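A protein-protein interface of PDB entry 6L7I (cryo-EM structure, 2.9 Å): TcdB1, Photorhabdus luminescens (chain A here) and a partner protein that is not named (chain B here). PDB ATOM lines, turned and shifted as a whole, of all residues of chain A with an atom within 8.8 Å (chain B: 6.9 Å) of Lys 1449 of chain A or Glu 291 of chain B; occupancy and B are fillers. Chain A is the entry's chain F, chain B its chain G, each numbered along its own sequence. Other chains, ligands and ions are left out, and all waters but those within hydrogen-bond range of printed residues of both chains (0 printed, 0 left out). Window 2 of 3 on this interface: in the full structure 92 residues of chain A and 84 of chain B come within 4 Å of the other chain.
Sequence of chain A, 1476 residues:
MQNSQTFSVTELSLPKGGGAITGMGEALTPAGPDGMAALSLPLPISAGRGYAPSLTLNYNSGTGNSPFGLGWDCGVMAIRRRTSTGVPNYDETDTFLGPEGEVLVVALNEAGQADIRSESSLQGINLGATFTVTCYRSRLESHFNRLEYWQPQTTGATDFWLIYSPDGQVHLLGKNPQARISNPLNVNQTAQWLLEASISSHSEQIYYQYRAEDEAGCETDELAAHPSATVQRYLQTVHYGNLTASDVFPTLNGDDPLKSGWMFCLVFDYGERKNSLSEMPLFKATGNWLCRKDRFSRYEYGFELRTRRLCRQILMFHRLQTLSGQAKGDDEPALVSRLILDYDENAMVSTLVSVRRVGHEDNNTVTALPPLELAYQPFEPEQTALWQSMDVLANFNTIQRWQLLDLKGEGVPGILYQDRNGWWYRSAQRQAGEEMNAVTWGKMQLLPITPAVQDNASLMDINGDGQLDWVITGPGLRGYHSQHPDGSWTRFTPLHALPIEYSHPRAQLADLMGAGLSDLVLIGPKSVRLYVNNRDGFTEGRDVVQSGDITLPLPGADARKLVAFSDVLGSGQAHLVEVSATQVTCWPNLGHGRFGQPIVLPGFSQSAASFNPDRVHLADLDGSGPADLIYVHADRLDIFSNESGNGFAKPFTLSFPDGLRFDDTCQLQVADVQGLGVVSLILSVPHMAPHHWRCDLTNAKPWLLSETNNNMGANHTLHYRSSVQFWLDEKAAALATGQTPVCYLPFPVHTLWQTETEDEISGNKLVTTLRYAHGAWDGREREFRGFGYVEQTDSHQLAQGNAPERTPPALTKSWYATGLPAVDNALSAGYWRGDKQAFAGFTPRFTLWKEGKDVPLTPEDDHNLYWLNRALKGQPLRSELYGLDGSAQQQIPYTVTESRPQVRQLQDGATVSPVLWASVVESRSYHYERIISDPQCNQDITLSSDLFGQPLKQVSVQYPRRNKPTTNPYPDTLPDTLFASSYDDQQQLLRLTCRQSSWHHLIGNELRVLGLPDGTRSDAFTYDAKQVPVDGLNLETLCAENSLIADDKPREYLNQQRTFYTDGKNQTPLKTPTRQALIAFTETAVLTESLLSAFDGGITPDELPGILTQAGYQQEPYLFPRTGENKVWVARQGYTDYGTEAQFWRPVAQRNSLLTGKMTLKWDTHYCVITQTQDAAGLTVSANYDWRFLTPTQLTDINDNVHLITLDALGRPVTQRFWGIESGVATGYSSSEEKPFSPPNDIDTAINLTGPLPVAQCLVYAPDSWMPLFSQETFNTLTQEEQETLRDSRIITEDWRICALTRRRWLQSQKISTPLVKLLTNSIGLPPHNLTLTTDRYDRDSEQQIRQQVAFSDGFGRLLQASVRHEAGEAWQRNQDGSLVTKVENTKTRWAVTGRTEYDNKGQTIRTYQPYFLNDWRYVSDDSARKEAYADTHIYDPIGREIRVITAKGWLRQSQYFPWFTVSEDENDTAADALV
Lys 1449 of chain A touches just these residues of chain B: Glu 291 (3.5 Å) and Glu 293 (3.9 Å).
Glu 291 of chain B touches just one residue of chain A: Lys 1449 (3.5 Å).
Of the printed residues of chain B, Gln 1410 of chain A touches Glu 293 and Gln 295.
Of the printed residues of chain A, Gln 295 of chain B touches Gln 1410 (3.3 Å).
Of the printed residues of chain B, Tyr 1430 of chain A touches Pro 292 (3.2 Å).
Of the printed residues of chain B, Ala 1448 of chain A touches Glu 293.
Gly 1450 of chain A touches none of the printed residues of chain B.
Ala 1431 of chain A touches none of the printed residues of chain B.
The nearest residue of chain B that does not touch Lys 1449 of chain A is Thr 294 of chain B (4.5 Å).
Gln 1410 of chain A touches Gln 295 of chain B.
Tyr 1430 of chain A touches Pro 292 of chain B (CE2 to O, 3.2 Å).
Ala 1448 of chain A touches Glu 293 of chain B.
Glu 291 of chain B touches Lys 1449 of chain A.
CA of Lys 1449 of chain A touches CG of Glu 293 of chain B, at 3.9 Å.
OD1 of Asp 1432 of chain A sits at hydrogen-bond distance from N of Ala 1448 of chain A (2.6 Å).
The side-chain amide nitrogen of Gln 295 of chain B is in hydrogen-bond range of the backbone carbonyl oxygen of Glu 291 of chain B (2.8 Å).
The backbone NH (N) of Glu 291 of chain B is in hydrogen-bond range of the backbone carbonyl oxygen (O) of Arg 296 of chain B.
NE2 of Gln 295 of chain B sits at hydrogen-bond distance from O of Pro 292 of chain B (2.7 Å).
The side-chain amide nitrogen (NE2) of Gln 1410 of chain A sits close to the backbone carbonyl oxygen (O) of Glu 293 of chain B, 3.4 Å away.
Hydrophobic or aromatic side chains of chain B that line the printed part of chain A: Pro 292.
Of the 14 printed residues of chain A, 4 touch a printed residue of chain B.
Hydrophobic or aromatic side chains of chain A within 4 Å of the printed part of chain B: Tyr 1430 and Ala 1448.
Among the printed residues, 6 pairs touch across the chains.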
ATOM      1  N   GLN A1410      33.711 -31.087   4.719  1.00  0.00           N
ATOM      2  CA  GLN A1410      32.334 -31.500   4.885  1.00  0.00           C
ATOM      3  C   GLN A1410      31.966 -32.463   3.759  1.00  0.00           C
ATOM      4  O   GLN A1410      32.520 -32.373   2.662  1.00  0.00           O
ATOM      5  CB  GLN A1410      31.410 -30.288   4.863  1.00  0.00           C
ATOM      6  CG  GLN A1410      31.847 -29.163   5.758  1.00  0.00           C
ATOM      7  CD  GLN A1410      31.778 -29.520   7.225  1.00  0.00           C
ATOM      8  OE1 GLN A1410      30.811 -30.119   7.684  1.00  0.00           O
ATOM      9  NE2 GLN A1410      32.808 -29.148   7.972  1.00  0.00           N
ATOM     10  N   PRO A1411      31.063 -33.408   4.009  1.00  0.00           N
ATOM     11  CA  PRO A1411      30.687 -34.354   2.957  1.00  0.00           C
ATOM     12  C   PRO A1411      29.898 -33.679   1.849  1.00  0.00           C
ATOM     13  O   PRO A1411      29.310 -32.610   2.024  1.00  0.00           O
ATOM     14  CB  PRO A1411      29.830 -35.386   3.693  1.00  0.00           C
ATOM     15  CG  PRO A1411      30.176 -35.225   5.119  1.00  0.00           C
ATOM     16  CD  PRO A1411      30.465 -33.781   5.300  1.00  0.00           C
ATOM     17  N   TYR A1430      34.159 -26.499   0.800  1.00  0.00           N
ATOM     18  CA  TYR A1430      34.588 -25.846   2.041  1.00  0.00           C
ATOM     19  C   TYR A1430      35.011 -26.821   3.136  1.00  0.00           C
ATOM     20  O   TYR A1430      34.368 -27.846   3.372  1.00  0.00           O
ATOM     21  CB  TYR A1430      33.453 -24.957   2.564  1.00  0.00           C
ATOM     22  CG  TYR A1430      32.085 -25.424   2.125  1.00  0.00           C
ATOM     23  CD1 TYR A1430      31.364 -24.712   1.175  1.00  0.00           C
ATOM     24  CD2 TYR A1430      31.531 -26.593   2.627  1.00  0.00           C
ATOM     25  CE1 TYR A1430      30.126 -25.140   0.754  1.00  0.00           C
ATOM     26  CE2 TYR A1430      30.306 -27.033   2.205  1.00  0.00           C
ATOM     27  CZ  TYR A1430      29.602 -26.301   1.275  1.00  0.00           C
ATOM     28  OH  TYR A1430      28.370 -26.742   0.858  1.00  0.00           O
ATOM     29  N   ALA A1431      36.105 -26.474   3.812  1.00  0.00           N
ATOM     30  CA  ALA A1431      36.740 -27.349   4.783  1.00  0.00           C
ATOM     31  C   ALA A1431      37.321 -26.512   5.908  1.00  0.00           C
ATOM     32  O   ALA A1431      37.407 -25.288   5.817  1.00  0.00           O
ATOM     33  CB  ALA A1431      37.848 -28.180   4.148  1.00  0.00           C
ATOM     34  N   ASP A1432      37.743 -27.192   6.967  1.00  0.00           N
ATOM     35  CA  ASP A1432      38.398 -26.550   8.094  1.00  0.00           C
ATOM     36  C   ASP A1432      39.895 -26.783   7.982  1.00  0.00           C
ATOM     37  O   ASP A1432      40.346 -27.930   8.035  1.00  0.00           O
ATOM     38  CB  ASP A1432      37.884 -27.107   9.419  1.00  0.00           C
ATOM     39  CG  ASP A1432      36.401 -26.923   9.587  1.00  0.00           C
ATOM     40  OD1 ASP A1432      35.834 -26.048   8.907  1.00  0.00           O
ATOM     41  OD2 ASP A1432      35.805 -27.641  10.414  1.00  0.00           O
ATOM     42  N   THR A1433      40.661 -25.709   7.838  1.00  0.00           N
ATOM     43  CA  THR A1433      42.109 -25.830   7.816  1.00  0.00           C
ATOM     44  C   THR A1433      42.674 -25.778   9.231  1.00  0.00           C
ATOM     45  O   THR A1433      42.176 -25.063  10.102  1.00  0.00           O
ATOM     46  CB  THR A1433      42.743 -24.748   6.942  1.00  0.00           C
ATOM     47  OG1 THR A1433      44.167 -24.807   7.065  1.00  0.00           O
ATOM     48  CG2 THR A1433      42.260 -23.364   7.321  1.00  0.00           C
ATOM     49  N   ILE A1446      40.964 -22.614  11.442  1.00  0.00           N
ATOM     50  CA  ILE A1446      40.031 -21.721  10.773  1.00  0.00           C
ATOM     51  C   ILE A1446      38.911 -22.581  10.210  1.00  0.00           C
ATOM     52  O   ILE A1446      39.155 -23.461   9.379  1.00  0.00           O
ATOM     53  CB  ILE A1446      40.713 -20.906   9.664  1.00  0.00           C
ATOM     54  CG1 ILE A1446      41.826 -20.014  10.223  1.00  0.00           C
ATOM     55  CG2 ILE A1446      39.697 -20.048   8.948  1.00  0.00           C
ATOM     56  CD1 ILE A1446      43.235 -20.592  10.119  1.00  0.00           C
ATOM     57  N   THR A1447      37.687 -22.336  10.666  1.00  0.00           N
ATOM     58  CA  THR A1447      36.560 -23.144  10.244  1.00  0.00           C
ATOM     59  C   THR A1447      36.170 -22.813   8.806  1.00  0.00           C
ATOM     60  O   THR A1447      36.693 -21.887   8.183  1.00  0.00           O
ATOM     61  CB  THR A1447      35.368 -22.939  11.174  1.00  0.00           C
ATOM     62  OG1 THR A1447      34.981 -21.563  11.164  1.00  0.00           O
ATOM     63  CG2 THR A1447      35.718 -23.348  12.585  1.00  0.00           C
ATOM     64  N   ALA A1448      35.235 -23.606   8.276  1.00  0.00           N
ATOM     65  CA  ALA A1448      34.833 -23.466   6.881  1.00  0.00           C
ATOM     66  C   ALA A1448      34.043 -22.187   6.655  1.00  0.00           C
ATOM     67  O   ALA A1448      34.139 -21.576   5.587  1.00  0.00           O
ATOM     68  CB  ALA A1448      34.017 -24.677   6.449  1.00  0.00           C
ATOM     69  N   LYS A1449      33.267 -21.757   7.648  1.00  0.00           N
ATOM     70  CA  LYS A1449      32.473 -20.549   7.479  1.00  0.00           C
ATOM     71  C   LYS A1449      33.309 -19.288   7.642  1.00  0.00           C
ATOM     72  O   LYS A1449      32.981 -18.255   7.050  1.00  0.00           O
ATOM     73  CB  LYS A1449      31.306 -20.542   8.462  1.00  0.00           C
ATOM     74  CG  LYS A1449      30.132 -19.704   8.006  1.00  0.00           C
ATOM     75  CD  LYS A1449      28.819 -20.283   8.483  1.00  0.00           C
ATOM     76  CE  LYS A1449      27.682 -19.318   8.217  1.00  0.00           C
ATOM     77  NZ  LYS A1449      27.991 -17.954   8.727  1.00  0.00           N
ATOM     78  N   GLY A1450      34.377 -19.342   8.426  1.00  0.00           N
ATOM     79  CA  GLY A1450      35.247 -18.193   8.543  1.00  0.00           C
ATOM     80  C   GLY A1450      35.670 -17.867   9.957  1.00  0.00           C
ATOM     81  O   GLY A1450      36.590 -17.073  10.160  1.00  0.00           O
ATOM     82  N   TRP A1451      35.008 -18.458  10.944  1.00  0.00           N
ATOM     83  CA  TRP A1451      35.423 -18.271  12.323  1.00  0.00           C
ATOM     84  C   TRP A1451      36.653 -19.117  12.606  1.00  0.00           C
ATOM     85  O   TRP A1451      37.039 -19.976  11.814  1.00  0.00           O
ATOM     86  CB  TRP A1451      34.298 -18.639  13.281  1.00  0.00           C
ATOM     87  CG  TRP A1451      33.041 -17.892  13.035  1.00  0.00           C
ATOM     88  CD1 TRP A1451      32.836 -16.553  13.183  1.00  0.00           C
ATOM     89  CD2 TRP A1451      31.802 -18.442  12.595  1.00  0.00           C
ATOM     90  NE1 TRP A1451      31.544 -16.234  12.860  1.00  0.00           N
ATOM     91  CE2 TRP A1451      30.887 -17.379  12.496  1.00  0.00           C
ATOM     92  CE3 TRP A1451      31.377 -19.732  12.272  1.00  0.00           C
ATOM     93  CZ2 TRP A1451      29.571 -17.568  12.092  1.00  0.00           C
ATOM     94  CZ3 TRP A1451      30.075 -19.918  11.873  1.00  0.00           C
ATOM     95  CH2 TRP A1451      29.184 -18.844  11.786  1.00  0.00           C
ATOM     96  N   LEU A1452      37.279 -18.877  13.752  1.00  0.00           N
ATOM     97  CA  LEU A1452      38.446 -19.672  14.092  1.00  0.00           C
ATOM     98  C   LEU A1452      38.547 -19.874  15.594  1.00  0.00           C
ATOM     99  O   LEU A1452      38.234 -18.976  16.378  1.00  0.00           O
ATOM    100  CB  LEU A1452      39.749 -19.056  13.559  1.00  0.00           C
ATOM    101  CG  LEU A1452      40.384 -17.810  14.176  1.00  0.00           C
ATOM    102  CD1 LEU A1452      41.857 -17.797  13.850  1.00  0.00           C
ATOM    103  CD2 LEU A1452      39.729 -16.545  13.651  1.00  0.00           C
ATOM    104  N   GLU A1467      35.067 -20.241  18.825  1.00  0.00           N
ATOM    105  CA  GLU A1467      34.662 -19.327  17.768  1.00  0.00           C
ATOM    106  C   GLU A1467      33.943 -18.094  18.286  1.00  0.00           C
ATOM    107  O   GLU A1467      33.735 -17.156  17.512  1.00  0.00           O
ATOM    108  CB  GLU A1467      33.771 -20.054  16.770  1.00  0.00           C
ATOM    109  CG  GLU A1467      34.422 -21.258  16.133  1.00  0.00           C
ATOM    110  CD  GLU A1467      34.019 -22.548  16.798  1.00  0.00           C
ATOM    111  OE1 GLU A1467      33.999 -22.599  18.043  1.00  0.00           O
ATOM    112  OE2 GLU A1467      33.713 -23.516  16.077  1.00  0.00           O
ATOM    113  N   SER B 289      16.572 -28.217   6.202  1.00  0.00           N
ATOM    114  CA  SER B 289      17.618 -27.435   5.570  1.00  0.00           C
ATOM    115  C   SER B 289      18.802 -27.327   6.516  1.00  0.00           C
ATOM    116  O   SER B 289      18.631 -27.263   7.733  1.00  0.00           O
ATOM    117  CB  SER B 289      17.112 -26.041   5.211  1.00  0.00           C
ATOM    118  OG  SER B 289      16.040 -26.117   4.295  1.00  0.00           O
ATOM    119  N   TYR B 290      20.006 -27.309   5.960  1.00  0.00           N
ATOM    120  CA  TYR B 290      21.208 -27.303   6.775  1.00  0.00           C
ATOM    121  C   TYR B 290      22.145 -26.203   6.317  1.00  0.00           C
ATOM    122  O   TYR B 290      22.029 -25.677   5.209  1.00  0.00           O
ATOM    123  CB  TYR B 290      21.949 -28.645   6.737  1.00  0.00           C
ATOM    124  CG  TYR B 290      21.113 -29.781   7.246  1.00  0.00           C
ATOM    125  CD1 TYR B 290      21.114 -30.122   8.590  1.00  0.00           C
ATOM    126  CD2 TYR B 290      20.304 -30.500   6.385  1.00  0.00           C
ATOM    127  CE1 TYR B 290      20.338 -31.153   9.056  1.00  0.00           C
ATOM    128  CE2 TYR B 290      19.529 -31.518   6.840  1.00  0.00           C
ATOM    129  CZ  TYR B 290      19.542 -31.840   8.172  1.00  0.00           C
ATOM    130  OH  TYR B 290      18.757 -32.874   8.613  1.00  0.00           O
ATOM    131  N   GLU B 291      23.058 -25.844   7.206  1.00  0.00           N
ATOM    132  CA  GLU B 291      24.156 -24.987   6.820  1.00  0.00           C
ATOM    133  C   GLU B 291      25.049 -25.741   5.847  1.00  0.00           C
ATOM    134  O   GLU B 291      25.258 -26.946   6.009  1.00  0.00           O
ATOM    135  CB  GLU B 291      24.970 -24.565   8.039  1.00  0.00           C
ATOM    136  CG  GLU B 291      24.637 -23.204   8.584  1.00  0.00           C
ATOM    137  CD  GLU B 291      25.077 -22.095   7.668  1.00  0.00           C
ATOM    138  OE1 GLU B 291      26.141 -22.239   7.037  1.00  0.00           O
ATOM    139  OE2 GLU B 291      24.351 -21.083   7.572  1.00  0.00           O
ATOM    140  N   PRO B 292      25.550 -25.093   4.819  1.00  0.00           N
ATOM    141  CA  PRO B 292      26.548 -25.741   3.968  1.00  0.00           C
ATOM    142  C   PRO B 292      27.848 -25.972   4.716  1.00  0.00           C
ATOM    143  O   PRO B 292      28.396 -27.074   4.716  1.00  0.00           O
ATOM    144  CB  PRO B 292      26.717 -24.745   2.816  1.00  0.00           C
ATOM    145  CG  PRO B 292      25.477 -23.935   2.828  1.00  0.00           C
ATOM    146  CD  PRO B 292      25.117 -23.804   4.264  1.00  0.00           C
ATOM    147  N   GLU B 293      28.318 -24.932   5.400  1.00  0.00           N
ATOM    148  CA  GLU B 293      29.657 -24.935   5.972  1.00  0.00           C
ATOM    149  C   GLU B 293      29.743 -25.761   7.248  1.00  0.00           C
ATOM    150  O   GLU B 293      30.688 -26.533   7.427  1.00  0.00           O
ATOM    151  CB  GLU B 293      30.101 -23.500   6.237  1.00  0.00           C
ATOM    152  CG  GLU B 293      30.448 -22.732   4.992  1.00  0.00           C
ATOM    153  CD  GLU B 293      29.276 -21.979   4.415  1.00  0.00           C
ATOM    154  OE1 GLU B 293      28.139 -22.198   4.872  1.00  0.00           O
ATOM    155  OE2 GLU B 293      29.492 -21.160   3.500  1.00  0.00           O
ATOM    156  N   THR B 294      28.789 -25.599   8.158  1.00  0.00           N
ATOM    157  CA  THR B 294      28.881 -26.226   9.467  1.00  0.00           C
ATOM    158  C   THR B 294      27.978 -27.440   9.625  1.00  0.00           C
ATOM    159  O   THR B 294      28.111 -28.147  10.628  1.00  0.00           O
ATOM    160  CB  THR B 294      28.557 -25.210  10.567  1.00  0.00           C
ATOM    161  OG1 THR B 294      27.324 -24.556  10.267  1.00  0.00           O
ATOM    162  CG2 THR B 294      29.639 -24.158  10.655  1.00  0.00           C
ATOM    163  N   GLN B 295      27.079 -27.683   8.664  1.00  0.00           N
ATOM    164  CA  GLN B 295      26.093 -28.776   8.677  1.00  0.00           C
ATOM    165  C   GLN B 295      25.194 -28.727   9.911  1.00  0.00           C
ATOM    166  O   GLN B 295      24.840 -29.758  10.480  1.00  0.00           O
ATOM    167  CB  GLN B 295      26.757 -30.148   8.544  1.00  0.00           C
ATOM    168  CG  GLN B 295      27.534 -30.341   7.258  1.00  0.00           C
ATOM    169  CD  GLN B 295      26.659 -30.286   6.032  1.00  0.00           C
ATOM    170  OE1 GLN B 295      25.874 -31.196   5.776  1.00  0.00           O
ATOM    171  NE2 GLN B 295      26.788 -29.214   5.262  1.00  0.00           N
ATOM    172  N   ARG B 296      24.801 -27.524  10.308  1.00  0.00           N
ATOM    173  CA  ARG B 296      23.865 -27.328  11.403  1.00  0.00           C
ATOM    174  C   ARG B 296      22.458 -27.148  10.856  1.00  0.00           C
ATOM    175  O   ARG B 296      22.267 -26.601   9.773  1.00  0.00           O
ATOM    176  CB  ARG B 296      24.257 -26.110  12.237  1.00  0.00           C
ATOM    177  CG  ARG B 296      25.655 -26.189  12.797  1.00  0.00           C
ATOM    178  CD  ARG B 296      25.737 -25.593  14.178  1.00  0.00           C
ATOM    179  NE  ARG B 296      25.993 -24.160  14.146  1.00  0.00           N
ATOM    180  CZ  ARG B 296      27.165 -23.609  14.429  1.00  0.00           C
ATOM    181  NH1 ARG B 296      28.192 -24.375  14.761  1.00  0.00           N
ATOM    182  NH2 ARG B 296      27.310 -22.294  14.377  1.00  0.00           N
ATOM    183  N   LEU B 297      21.471 -27.605  11.620  1.00  0.00           N
ATOM    184  CA  LEU B 297      20.081 -27.554  11.187  1.00  0.00           C
ATOM    185  C   LEU B 297      19.575 -26.121  11.242  1.00  0.00           C
ATOM    186  O   LEU B 297      19.482 -25.528  12.319  1.00  0.00           O
ATOM    187  CB  LEU B 297      19.216 -28.457  12.058  1.00  0.00           C
ATOM    188  CG  LEU B 297      17.744 -28.551  11.663  1.00  0.00           C
ATOM    189  CD1 LEU B 297      17.607 -29.160  10.292  1.00  0.00           C
ATOM    190  CD2 LEU B 297      16.963 -29.356  12.673  1.00  0.00           C
ATOM    191  N   ILE B 298      19.247 -25.567  10.080  1.00  0.00           N
ATOM    192  CA  ILE B 298      18.791 -24.192   9.965  1.00  0.00           C
ATOM    193  C   ILE B 298      17.367 -24.102   9.438  1.00  0.00           C
ATOM    194  O   ILE B 298      16.910 -23.017   9.089  1.00  0.00           O
ATOM    195  CB  ILE B 298      19.745 -23.365   9.085  1.00  0.00           C
ATOM    196  CG1 ILE B 298      19.787 -23.935   7.673  1.00  0.00           C
ATOM    197  CG2 ILE B 298      21.121 -23.361   9.673  1.00  0.00           C
ATOM    198  CD1 ILE B 298      20.443 -23.029   6.677  1.00  0.00           C
ATOM    199  N   GLY B 299      16.656 -25.218   9.367  1.00  0.00           N
ATOM    200  CA  GLY B 299      15.298 -25.177   8.876  1.00  0.00           C
ATOM    201  C   GLY B 299      14.538 -26.471   9.035  1.00  0.00           C
ATOM    202  O   GLY B 299      15.058 -27.540   8.718  1.00  0.00           O
ATOM    203  N   TYR B 318      22.191 -19.031  14.812  1.00  0.00           N
ATOM    204  CA  TYR B 318      23.160 -19.564  15.750  1.00  0.00           C
ATOM    205  C   TYR B 318      24.203 -18.520  16.108  1.00  0.00           C
ATOM    206  O   TYR B 318      24.328 -17.476  15.468  1.00  0.00           O
ATOM    207  CB  TYR B 318      23.858 -20.799  15.178  1.00  0.00           C
ATOM    208  CG  TYR B 318      22.980 -22.016  15.068  1.00  0.00           C
ATOM    209  CD1 TYR B 318      22.202 -22.235  13.944  1.00  0.00           C
ATOM    210  CD2 TYR B 318      22.947 -22.957  16.081  1.00  0.00           C
ATOM    211  CE1 TYR B 318      21.405 -23.348  13.839  1.00  0.00           C
ATOM    212  CE2 TYR B 318      22.158 -24.074  15.984  1.00  0.00           C
ATOM    213  CZ  TYR B 318      21.388 -24.263  14.863  1.00  0.00           C
ATOM    214  OH  TYR B 318      20.601 -25.381  14.769  1.00  0.00           O
